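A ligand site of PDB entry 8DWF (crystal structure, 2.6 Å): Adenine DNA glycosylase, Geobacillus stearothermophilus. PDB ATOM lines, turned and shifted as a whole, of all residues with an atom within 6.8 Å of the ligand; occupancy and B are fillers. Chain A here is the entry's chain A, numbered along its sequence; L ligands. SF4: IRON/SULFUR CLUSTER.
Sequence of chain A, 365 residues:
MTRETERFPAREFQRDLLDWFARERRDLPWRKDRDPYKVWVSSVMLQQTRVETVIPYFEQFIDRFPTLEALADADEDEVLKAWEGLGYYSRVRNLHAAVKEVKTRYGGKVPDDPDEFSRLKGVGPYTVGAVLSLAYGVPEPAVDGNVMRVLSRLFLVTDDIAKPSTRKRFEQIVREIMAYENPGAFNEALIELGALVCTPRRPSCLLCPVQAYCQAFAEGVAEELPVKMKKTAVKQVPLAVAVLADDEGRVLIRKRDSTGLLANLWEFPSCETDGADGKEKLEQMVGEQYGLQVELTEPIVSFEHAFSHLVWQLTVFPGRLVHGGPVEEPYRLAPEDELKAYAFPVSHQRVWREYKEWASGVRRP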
ATOM      1  N   ARG A 149       3.012 -28.458  12.680  1.00  0.00           N
ATOM      2  CA  ARG A 149       2.898 -27.181  13.385  1.00  0.00           C
ATOM      3  C   ARG A 149       4.179 -26.830  14.115  1.00  0.00           C
ATOM      4  O   ARG A 149       4.630 -25.689  14.066  1.00  0.00           O
ATOM      5  CB  ARG A 149       1.696 -27.253  14.324  1.00  0.00           C
ATOM      6  CG  ARG A 149       1.697 -26.269  15.443  1.00  0.00           C
ATOM      7  CD  ARG A 149       0.309 -26.108  16.103  1.00  0.00           C
ATOM      8  NE  ARG A 149      -0.534 -27.294  16.008  1.00  0.00           N
ATOM      9  CZ  ARG A 149      -0.428 -28.334  16.810  1.00  0.00           C
ATOM     10  NH1 ARG A 149       0.496 -28.384  17.751  1.00  0.00           N
ATOM     11  NH2 ARG A 149      -1.250 -29.378  16.651  1.00  0.00           N
ATOM     12  N   VAL A 150       4.833 -27.807  14.754  1.00  0.00           N
ATOM     13  CA  VAL A 150       6.111 -27.543  15.400  1.00  0.00           C
ATOM     14  C   VAL A 150       7.199 -27.193  14.382  1.00  0.00           C
ATOM     15  O   VAL A 150       7.983 -26.269  14.600  1.00  0.00           O
ATOM     16  CB  VAL A 150       6.538 -28.742  16.264  1.00  0.00           C
ATOM     17  CG1 VAL A 150       8.016 -28.540  16.839  1.00  0.00           C
ATOM     18  CG2 VAL A 150       5.544 -28.953  17.358  1.00  0.00           C
ATOM     19  N   ARG A 153       6.886 -23.817  12.628  1.00  0.00           N
ATOM     20  CA  ARG A 153       7.299 -22.729  13.532  1.00  0.00           C
ATOM     21  C   ARG A 153       8.825 -22.731  13.752  1.00  0.00           C
ATOM     22  O   ARG A 153       9.466 -21.665  13.714  1.00  0.00           O
ATOM     23  CB  ARG A 153       6.540 -22.859  14.865  1.00  0.00           C
ATOM     24  CG  ARG A 153       5.115 -22.383  14.786  1.00  0.00           C
ATOM     25  CD  ARG A 153       4.317 -22.806  15.963  1.00  0.00           C
ATOM     26  NE  ARG A 153       2.943 -22.323  15.889  1.00  0.00           N
ATOM     27  CZ  ARG A 153       1.982 -22.707  16.718  1.00  0.00           C
ATOM     28  NH1 ARG A 153       2.229 -23.567  17.696  1.00  0.00           N
ATOM     29  NH2 ARG A 153       0.754 -22.231  16.557  1.00  0.00           N
ATOM     30  N   LEU A 154       9.426 -23.891  13.963  1.00  0.00           N
ATOM     31  CA  LEU A 154      10.863 -23.940  14.100  1.00  0.00           C
ATOM     32  C   LEU A 154      11.573 -23.423  12.868  1.00  0.00           C
ATOM     33  O   LEU A 154      12.625 -22.775  12.984  1.00  0.00           O
ATOM     34  CB  LEU A 154      11.312 -25.362  14.372  1.00  0.00           C
ATOM     35  CG  LEU A 154      10.999 -25.823  15.787  1.00  0.00           C
ATOM     36  CD1 LEU A 154      11.349 -27.284  15.907  1.00  0.00           C
ATOM     37  CD2 LEU A 154      11.764 -25.033  16.845  1.00  0.00           C
ATOM     38  N   LEU A 193       5.521 -32.422  21.928  1.00  0.00           N
ATOM     39  CA  LEU A 193       5.769 -31.005  22.077  1.00  0.00           C
ATOM     40  C   LEU A 193       4.682 -30.201  21.431  1.00  0.00           C
ATOM     41  O   LEU A 193       4.255 -29.197  21.985  1.00  0.00           O
ATOM     42  CB  LEU A 193       7.135 -30.644  21.486  1.00  0.00           C
ATOM     43  CG  LEU A 193       7.582 -29.196  21.551  1.00  0.00           C
ATOM     44  CD1 LEU A 193       7.631 -28.685  22.955  1.00  0.00           C
ATOM     45  CD2 LEU A 193       8.954 -29.167  20.900  1.00  0.00           C
ATOM     46  N   VAL A 197       2.869 -28.068  24.361  1.00  0.00           N
ATOM     47  CA  VAL A 197       3.582 -26.800  24.443  1.00  0.00           C
ATOM     48  C   VAL A 197       3.364 -25.961  23.197  1.00  0.00           C
ATOM     49  O   VAL A 197       2.838 -24.839  23.257  1.00  0.00           O
ATOM     50  CB  VAL A 197       5.080 -27.056  24.673  1.00  0.00           C
ATOM     51  CG1 VAL A 197       5.890 -25.751  24.736  1.00  0.00           C
ATOM     52  CG2 VAL A 197       5.269 -27.864  25.914  1.00  0.00           C
ATOM     53  N   CYS A 198       3.841 -26.475  22.067  1.00  0.00           N
ATOM     54  CA  CYS A 198       3.669 -25.776  20.783  1.00  0.00           C
ATOM     55  C   CYS A 198       2.250 -26.020  20.265  1.00  0.00           C
ATOM     56  O   CYS A 198       2.016 -26.626  19.211  1.00  0.00           O
ATOM     57  CB  CYS A 198       4.753 -26.223  19.802  1.00  0.00           C
ATOM     58  SG  CYS A 198       4.929 -25.127  18.378  1.00  0.00           S
ATOM     59  N   THR A 199       1.278 -25.527  21.049  1.00  0.00           N
ATOM     60  CA  THR A 199      -0.133 -25.786  20.782  1.00  0.00           C
ATOM     61  C   THR A 199      -0.625 -24.899  19.630  1.00  0.00           C
ATOM     62  O   THR A 199       0.060 -23.974  19.187  1.00  0.00           O
ATOM     63  CB  THR A 199      -0.963 -25.594  22.061  1.00  0.00           C
ATOM     64  OG1 THR A 199      -0.876 -24.249  22.564  1.00  0.00           O
ATOM     65  CG2 THR A 199      -0.475 -26.525  23.146  1.00  0.00           C
ATOM     66  N   PRO A 203       0.595 -20.763  21.841  1.00  0.00           N
ATOM     67  CA  PRO A 203       1.643 -21.724  22.244  1.00  0.00           C
ATOM     68  C   PRO A 203       2.438 -21.235  23.460  1.00  0.00           C
ATOM     69  O   PRO A 203       2.554 -20.034  23.713  1.00  0.00           O
ATOM     70  CB  PRO A 203       2.517 -21.843  20.988  1.00  0.00           C
ATOM     71  CG  PRO A 203       2.250 -20.645  20.212  1.00  0.00           C
ATOM     72  CD  PRO A 203       0.839 -20.238  20.490  1.00  0.00           C
ATOM     73  N   SER A 204       2.965 -22.200  24.212  1.00  0.00           N
ATOM     74  CA  SER A 204       3.655 -21.923  25.474  1.00  0.00           C
ATOM     75  C   SER A 204       5.143 -21.680  25.270  1.00  0.00           C
ATOM     76  O   SER A 204       5.969 -22.259  25.967  1.00  0.00           O
ATOM     77  CB  SER A 204       3.445 -23.059  26.475  1.00  0.00           C
ATOM     78  OG  SER A 204       2.071 -23.387  26.651  1.00  0.00           O
ATOM     79  N   CYS A 205       5.458 -20.761  24.353  1.00  0.00           N
ATOM     80  CA  CYS A 205       6.839 -20.548  23.927  1.00  0.00           C
ATOM     81  C   CYS A 205       7.796 -20.305  25.107  1.00  0.00           C
ATOM     82  O   CYS A 205       8.946 -20.756  25.100  1.00  0.00           O
ATOM     83  CB  CYS A 205       6.873 -19.385  22.952  1.00  0.00           C
ATOM     84  SG  CYS A 205       5.858 -19.616  21.492  1.00  0.00           S
ATOM     85  N   LEU A 206       7.349 -19.574  26.119  1.00  0.00           N
ATOM     86  CA  LEU A 206       8.192 -19.328  27.293  1.00  0.00           C
ATOM     87  C   LEU A 206       8.290 -20.546  28.213  1.00  0.00           C
ATOM     88  O   LEU A 206       8.943 -20.468  29.252  1.00  0.00           O
ATOM     89  CB  LEU A 206       7.664 -18.104  28.078  1.00  0.00           C
ATOM     90  CG  LEU A 206       7.613 -16.766  27.315  1.00  0.00           C
ATOM     91  CD1 LEU A 206       6.479 -15.874  27.817  1.00  0.00           C
ATOM     92  CD2 LEU A 206       8.981 -16.010  27.356  1.00  0.00           C
ATOM     93  N   LEU A 207       7.632 -21.640  27.858  1.00  0.00           N
ATOM     94  CA  LEU A 207       7.696 -22.894  28.592  1.00  0.00           C
ATOM     95  C   LEU A 207       8.315 -24.006  27.758  1.00  0.00           C
ATOM     96  O   LEU A 207       8.168 -25.184  28.102  1.00  0.00           O
ATOM     97  CB  LEU A 207       6.297 -23.337  29.004  1.00  0.00           C
ATOM     98  CG  LEU A 207       5.912 -23.202  30.451  1.00  0.00           C
ATOM     99  CD1 LEU A 207       4.487 -23.692  30.574  1.00  0.00           C
ATOM    100  CD2 LEU A 207       6.887 -23.990  31.319  1.00  0.00           C
ATOM    101  N   CYS A 208       8.910 -23.642  26.631  1.00  0.00           N
ATOM    102  CA  CYS A 208       9.368 -24.533  25.586  1.00  0.00           C
ATOM    103  C   CYS A 208      10.839 -24.833  25.767  1.00  0.00           C
ATOM    104  O   CYS A 208      11.659 -23.925  25.976  1.00  0.00           O
ATOM    105  CB  CYS A 208       9.120 -23.896  24.228  1.00  0.00           C
ATOM    106  SG  CYS A 208       9.580 -24.988  22.917  1.00  0.00           S
ATOM    107  N   PRO A 209      11.220 -26.100  25.692  1.00  0.00           N
ATOM    108  CA  PRO A 209      12.644 -26.466  25.789  1.00  0.00           C
ATOM    109  C   PRO A 209      13.452 -26.122  24.546  1.00  0.00           C
ATOM    110  O   PRO A 209      14.689 -26.231  24.611  1.00  0.00           O
ATOM    111  CB  PRO A 209      12.613 -27.990  25.986  1.00  0.00           C
ATOM    112  CG  PRO A 209      11.384 -28.432  25.232  1.00  0.00           C
ATOM    113  CD  PRO A 209      10.346 -27.280  25.465  1.00  0.00           C
ATOM    114  N   VAL A 210      12.821 -25.763  23.417  1.00  0.00           N
ATOM    115  CA  VAL A 210      13.538 -25.562  22.158  1.00  0.00           C
ATOM    116  C   VAL A 210      13.230 -24.173  21.635  1.00  0.00           C
ATOM    117  O   VAL A 210      13.207 -23.920  20.442  1.00  0.00           O
ATOM    118  CB  VAL A 210      13.215 -26.652  21.107  1.00  0.00           C
ATOM    119  CG1 VAL A 210      13.815 -28.001  21.558  1.00  0.00           C
ATOM    120  CG2 VAL A 210      11.691 -26.803  20.785  1.00  0.00           C
ATOM    121  N   GLN A 211      13.025 -23.241  22.547  1.00  0.00           N
ATOM    122  CA  GLN A 211      12.742 -21.863  22.159  1.00  0.00           C
ATOM    123  C   GLN A 211      13.932 -21.201  21.454  1.00  0.00           C
ATOM    124  O   GLN A 211      13.762 -20.362  20.553  1.00  0.00           O
ATOM    125  CB  GLN A 211      12.351 -21.114  23.411  1.00  0.00           C
ATOM    126  CG  GLN A 211      12.012 -19.690  23.242  1.00  0.00           C
ATOM    127  CD  GLN A 211      11.793 -19.086  24.582  1.00  0.00           C
ATOM    128  OE1 GLN A 211      10.692 -18.702  24.933  1.00  0.00           O
ATOM    129  NE2 GLN A 211      12.849 -19.054  25.379  1.00  0.00           N
ATOM    130  N   ALA A 212      15.132 -21.570  21.862  1.00  0.00           N
ATOM    131  CA  ALA A 212      16.311 -20.992  21.223  1.00  0.00           C
ATOM    132  C   ALA A 212      16.418 -21.366  19.744  1.00  0.00           C
ATOM    133  O   ALA A 212      17.047 -20.635  18.975  1.00  0.00           O
ATOM    134  CB  ALA A 212      17.582 -21.467  21.917  1.00  0.00           C
ATOM    135  N   TYR A 213      15.886 -22.516  19.351  1.00  0.00           N
ATOM    136  CA  TYR A 213      16.047 -22.964  17.985  1.00  0.00           C
ATOM    137  C   TYR A 213      14.879 -22.555  17.109  1.00  0.00           C
ATOM    138  O   TYR A 213      14.901 -22.867  15.915  1.00  0.00           O
ATOM    139  CB  TYR A 213      16.246 -24.471  17.977  1.00  0.00           C
ATOM    140  CG  TYR A 213      17.204 -24.938  19.053  1.00  0.00           C
ATOM    141  CD1 TYR A 213      18.575 -24.777  18.930  1.00  0.00           C
ATOM    142  CD2 TYR A 213      16.731 -25.555  20.198  1.00  0.00           C
ATOM    143  CE1 TYR A 213      19.441 -25.230  19.911  1.00  0.00           C
ATOM    144  CE2 TYR A 213      17.588 -25.997  21.176  1.00  0.00           C
ATOM    145  CZ  TYR A 213      18.925 -25.848  21.047  1.00  0.00           C
ATOM    146  OH  TYR A 213      19.725 -26.314  22.072  1.00  0.00           O
ATOM    147  N   CYS A 214      13.923 -21.793  17.648  1.00  0.00           N
ATOM    148  CA  CYS A 214      12.660 -21.527  16.982  1.00  0.00           C
ATOM    149  C   CYS A 214      12.766 -20.247  16.184  1.00  0.00           C
ATOM    150  O   CYS A 214      13.093 -19.194  16.744  1.00  0.00           O
ATOM    151  CB  CYS A 214      11.538 -21.427  17.996  1.00  0.00           C
ATOM    152  SG  CYS A 214       9.880 -21.391  17.298  1.00  0.00           S
ATOM    153  N   GLN A 215      12.495 -20.324  14.885  1.00  0.00           N
ATOM    154  CA  GLN A 215      12.551 -19.134  14.048  1.00  0.00           C
ATOM    155  C   GLN A 215      11.251 -18.347  14.106  1.00  0.00           C
ATOM    156  O   GLN A 215      11.277 -17.139  13.890  1.00  0.00           O
ATOM    157  CB  GLN A 215      12.858 -19.497  12.580  1.00  0.00           C
ATOM    158  CG  GLN A 215      14.266 -19.984  12.366  1.00  0.00           C
ATOM    159  CD  GLN A 215      14.503 -20.374  10.940  1.00  0.00           C
ATOM    160  OE1 GLN A 215      14.000 -19.729  10.001  1.00  0.00           O
ATOM    161  NE2 GLN A 215      15.263 -21.481  10.750  1.00  0.00           N
ATOM    162  N   ALA A 216      10.121 -19.001  14.349  1.00  0.00           N
ATOM    163  CA  ALA A 216       8.873 -18.262  14.467  1.00  0.00           C
ATOM    164  C   ALA A 216       8.803 -17.516  15.793  1.00  0.00           C
ATOM    165  O   ALA A 216       8.170 -16.467  15.877  1.00  0.00           O
ATOM    166  CB  ALA A 216       7.669 -19.194  14.338  1.00  0.00           C
ATOM    167  N   PHE A 217       9.455 -18.048  16.823  1.00  0.00           N
ATOM    168  CA  PHE A 217       9.569 -17.314  18.072  1.00  0.00           C
ATOM    169  C   PHE A 217      10.334 -16.015  17.850  1.00  0.00           C
ATOM    170  O   PHE A 217       9.910 -14.943  18.285  1.00  0.00           O
ATOM    171  CB  PHE A 217      10.250 -18.201  19.121  1.00  0.00           C
ATOM    172  CG  PHE A 217      10.493 -17.514  20.425  1.00  0.00           C
ATOM    173  CD1 PHE A 217       9.434 -17.212  21.275  1.00  0.00           C
ATOM    174  CD2 PHE A 217      11.768 -17.191  20.820  1.00  0.00           C
ATOM    175  CE1 PHE A 217       9.663 -16.574  22.477  1.00  0.00           C
ATOM    176  CE2 PHE A 217      12.002 -16.557  22.029  1.00  0.00           C
ATOM    177  CZ  PHE A 217      10.960 -16.254  22.855  1.00  0.00           C
ATOM    178  N   ALA A 222       4.552 -16.957  15.386  1.00  0.00           N
ATOM    179  CA  ALA A 222       4.143 -18.301  15.755  1.00  0.00           C
ATOM    180  C   ALA A 222       2.646 -18.505  15.589  1.00  0.00           C
ATOM    181  O   ALA A 222       2.209 -19.517  15.009  1.00  0.00           O
ATOM    182  CB  ALA A 222       4.556 -18.599  17.205  1.00  0.00           C
ATOM    183  N   GLU A 223       1.838 -17.575  16.097  1.00  0.00           N
ATOM    184  CA  GLU A 223       0.389 -17.682  16.012  1.00  0.00           C
ATOM    185  C   GLU A 223      -0.114 -17.764  14.570  1.00  0.00           C
ATOM    186  O   GLU A 223      -1.195 -18.300  14.311  1.00  0.00           O
ATOM    187  CB  GLU A 223      -0.212 -16.464  16.705  1.00  0.00           C
ATOM    188  CG  GLU A 223       0.001 -16.413  18.208  1.00  0.00           C
ATOM    189  CD  GLU A 223      -1.009 -17.268  18.962  1.00  0.00           C
ATOM    190  OE1 GLU A 223      -1.411 -18.345  18.436  1.00  0.00           O
ATOM    191  OE2 GLU A 223      -1.425 -16.865  20.081  1.00  0.00           O
HETATM  192 FE1  SF4 L   1       8.481 -23.664  21.215  1.00  0.00          FE
HETATM  193 FE2  SF4 L   1       6.845 -21.491  20.771  1.00  0.00          FE
HETATM  194 FE3  SF4 L   1       6.388 -23.762  19.463  1.00  0.00          FE
HETATM  195 FE4  SF4 L   1       8.551 -22.356  18.839  1.00  0.00          FE
HETATM  196  S1  SF4 L   1       6.366 -21.646  18.651  1.00  0.00           S
HETATM  197  S2  SF4 L   1       8.506 -24.567  19.137  1.00  0.00           S
HETATM  198  S3  SF4 L   1       9.148 -21.572  20.861  1.00  0.00           S
HETATM  199  S4  SF4 L   1       6.247 -23.535  21.683  1.00  0.00           S
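SG of Cys 208 lies close to N of Val 210, at 3.4 Å.
The backbone carbonyl oxygen (O) of Thr 199 is in hydrogen-bond range of the guanidinium group (NH1) of Arg 153.
The side-chain sulfur of Cys 214 lies close to the backbone carbonyl oxygen of Arg 153, 3.6 Å away.
The backbone NH (N) of Cys 198 sits at hydrogen-bond distance from the backbone carbonyl oxygen (O) of Leu 193 (2.8 Å).
The backbone carbonyl oxygen of Arg 153 sits at hydrogen-bond distance from the backbone NH of Ala 216, at 2.8 Å.
The backbone carbonyl oxygen (O) of Cys 198 is in hydrogen-bond range of the guanidinium group (NH1) of Arg 153, 3.4 Å away.
The side-chain sulfur (SG) of Cys 214 sits close to the backbone NH (N) of Phe 217 (3.4 Å).
The backbone carbonyl oxygen (O) of Cys 198 sits at hydrogen-bond distance from the guanidinium group (NH1) of Arg 149.
FE4 of the ligand is bound by SG of Cys 214 (2.3 Å).
SG of Cys 208 is bound to FE1 of the ligand, at 2.4 Å.
The side-chain sulfur (SG) of Cys 198 binds an iron atom (FE3) of the ligand, at 2.3 Å.
The side-chain sulfur of Cys 205 is bound to an iron atom (FE2) of the ligand.
CD of Arg 153 touches S1 of the ligand (3.6 Å).
Val 197 touches the ligand.
Gln 211 touches the ligand.
Phe 217 touches the ligand (CB to S3, 3.95 Å).
Ala 222 touches the ligand (CB to S1, 3.8 Å).
Hydrophobic or aromatic side chains that line the ligand: Val 197, Phe 217 and Ala 222.
Nine residues have an atom within 4 Å of the ligand: Arg 153, Val 197, Cys 198, Cys 205, Cys 208, Gln 211, Cys 214, Phe 217 and Ala 222.
The nearest printed residue that does not touch the ligand is Leu 154 (4.01 Å).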
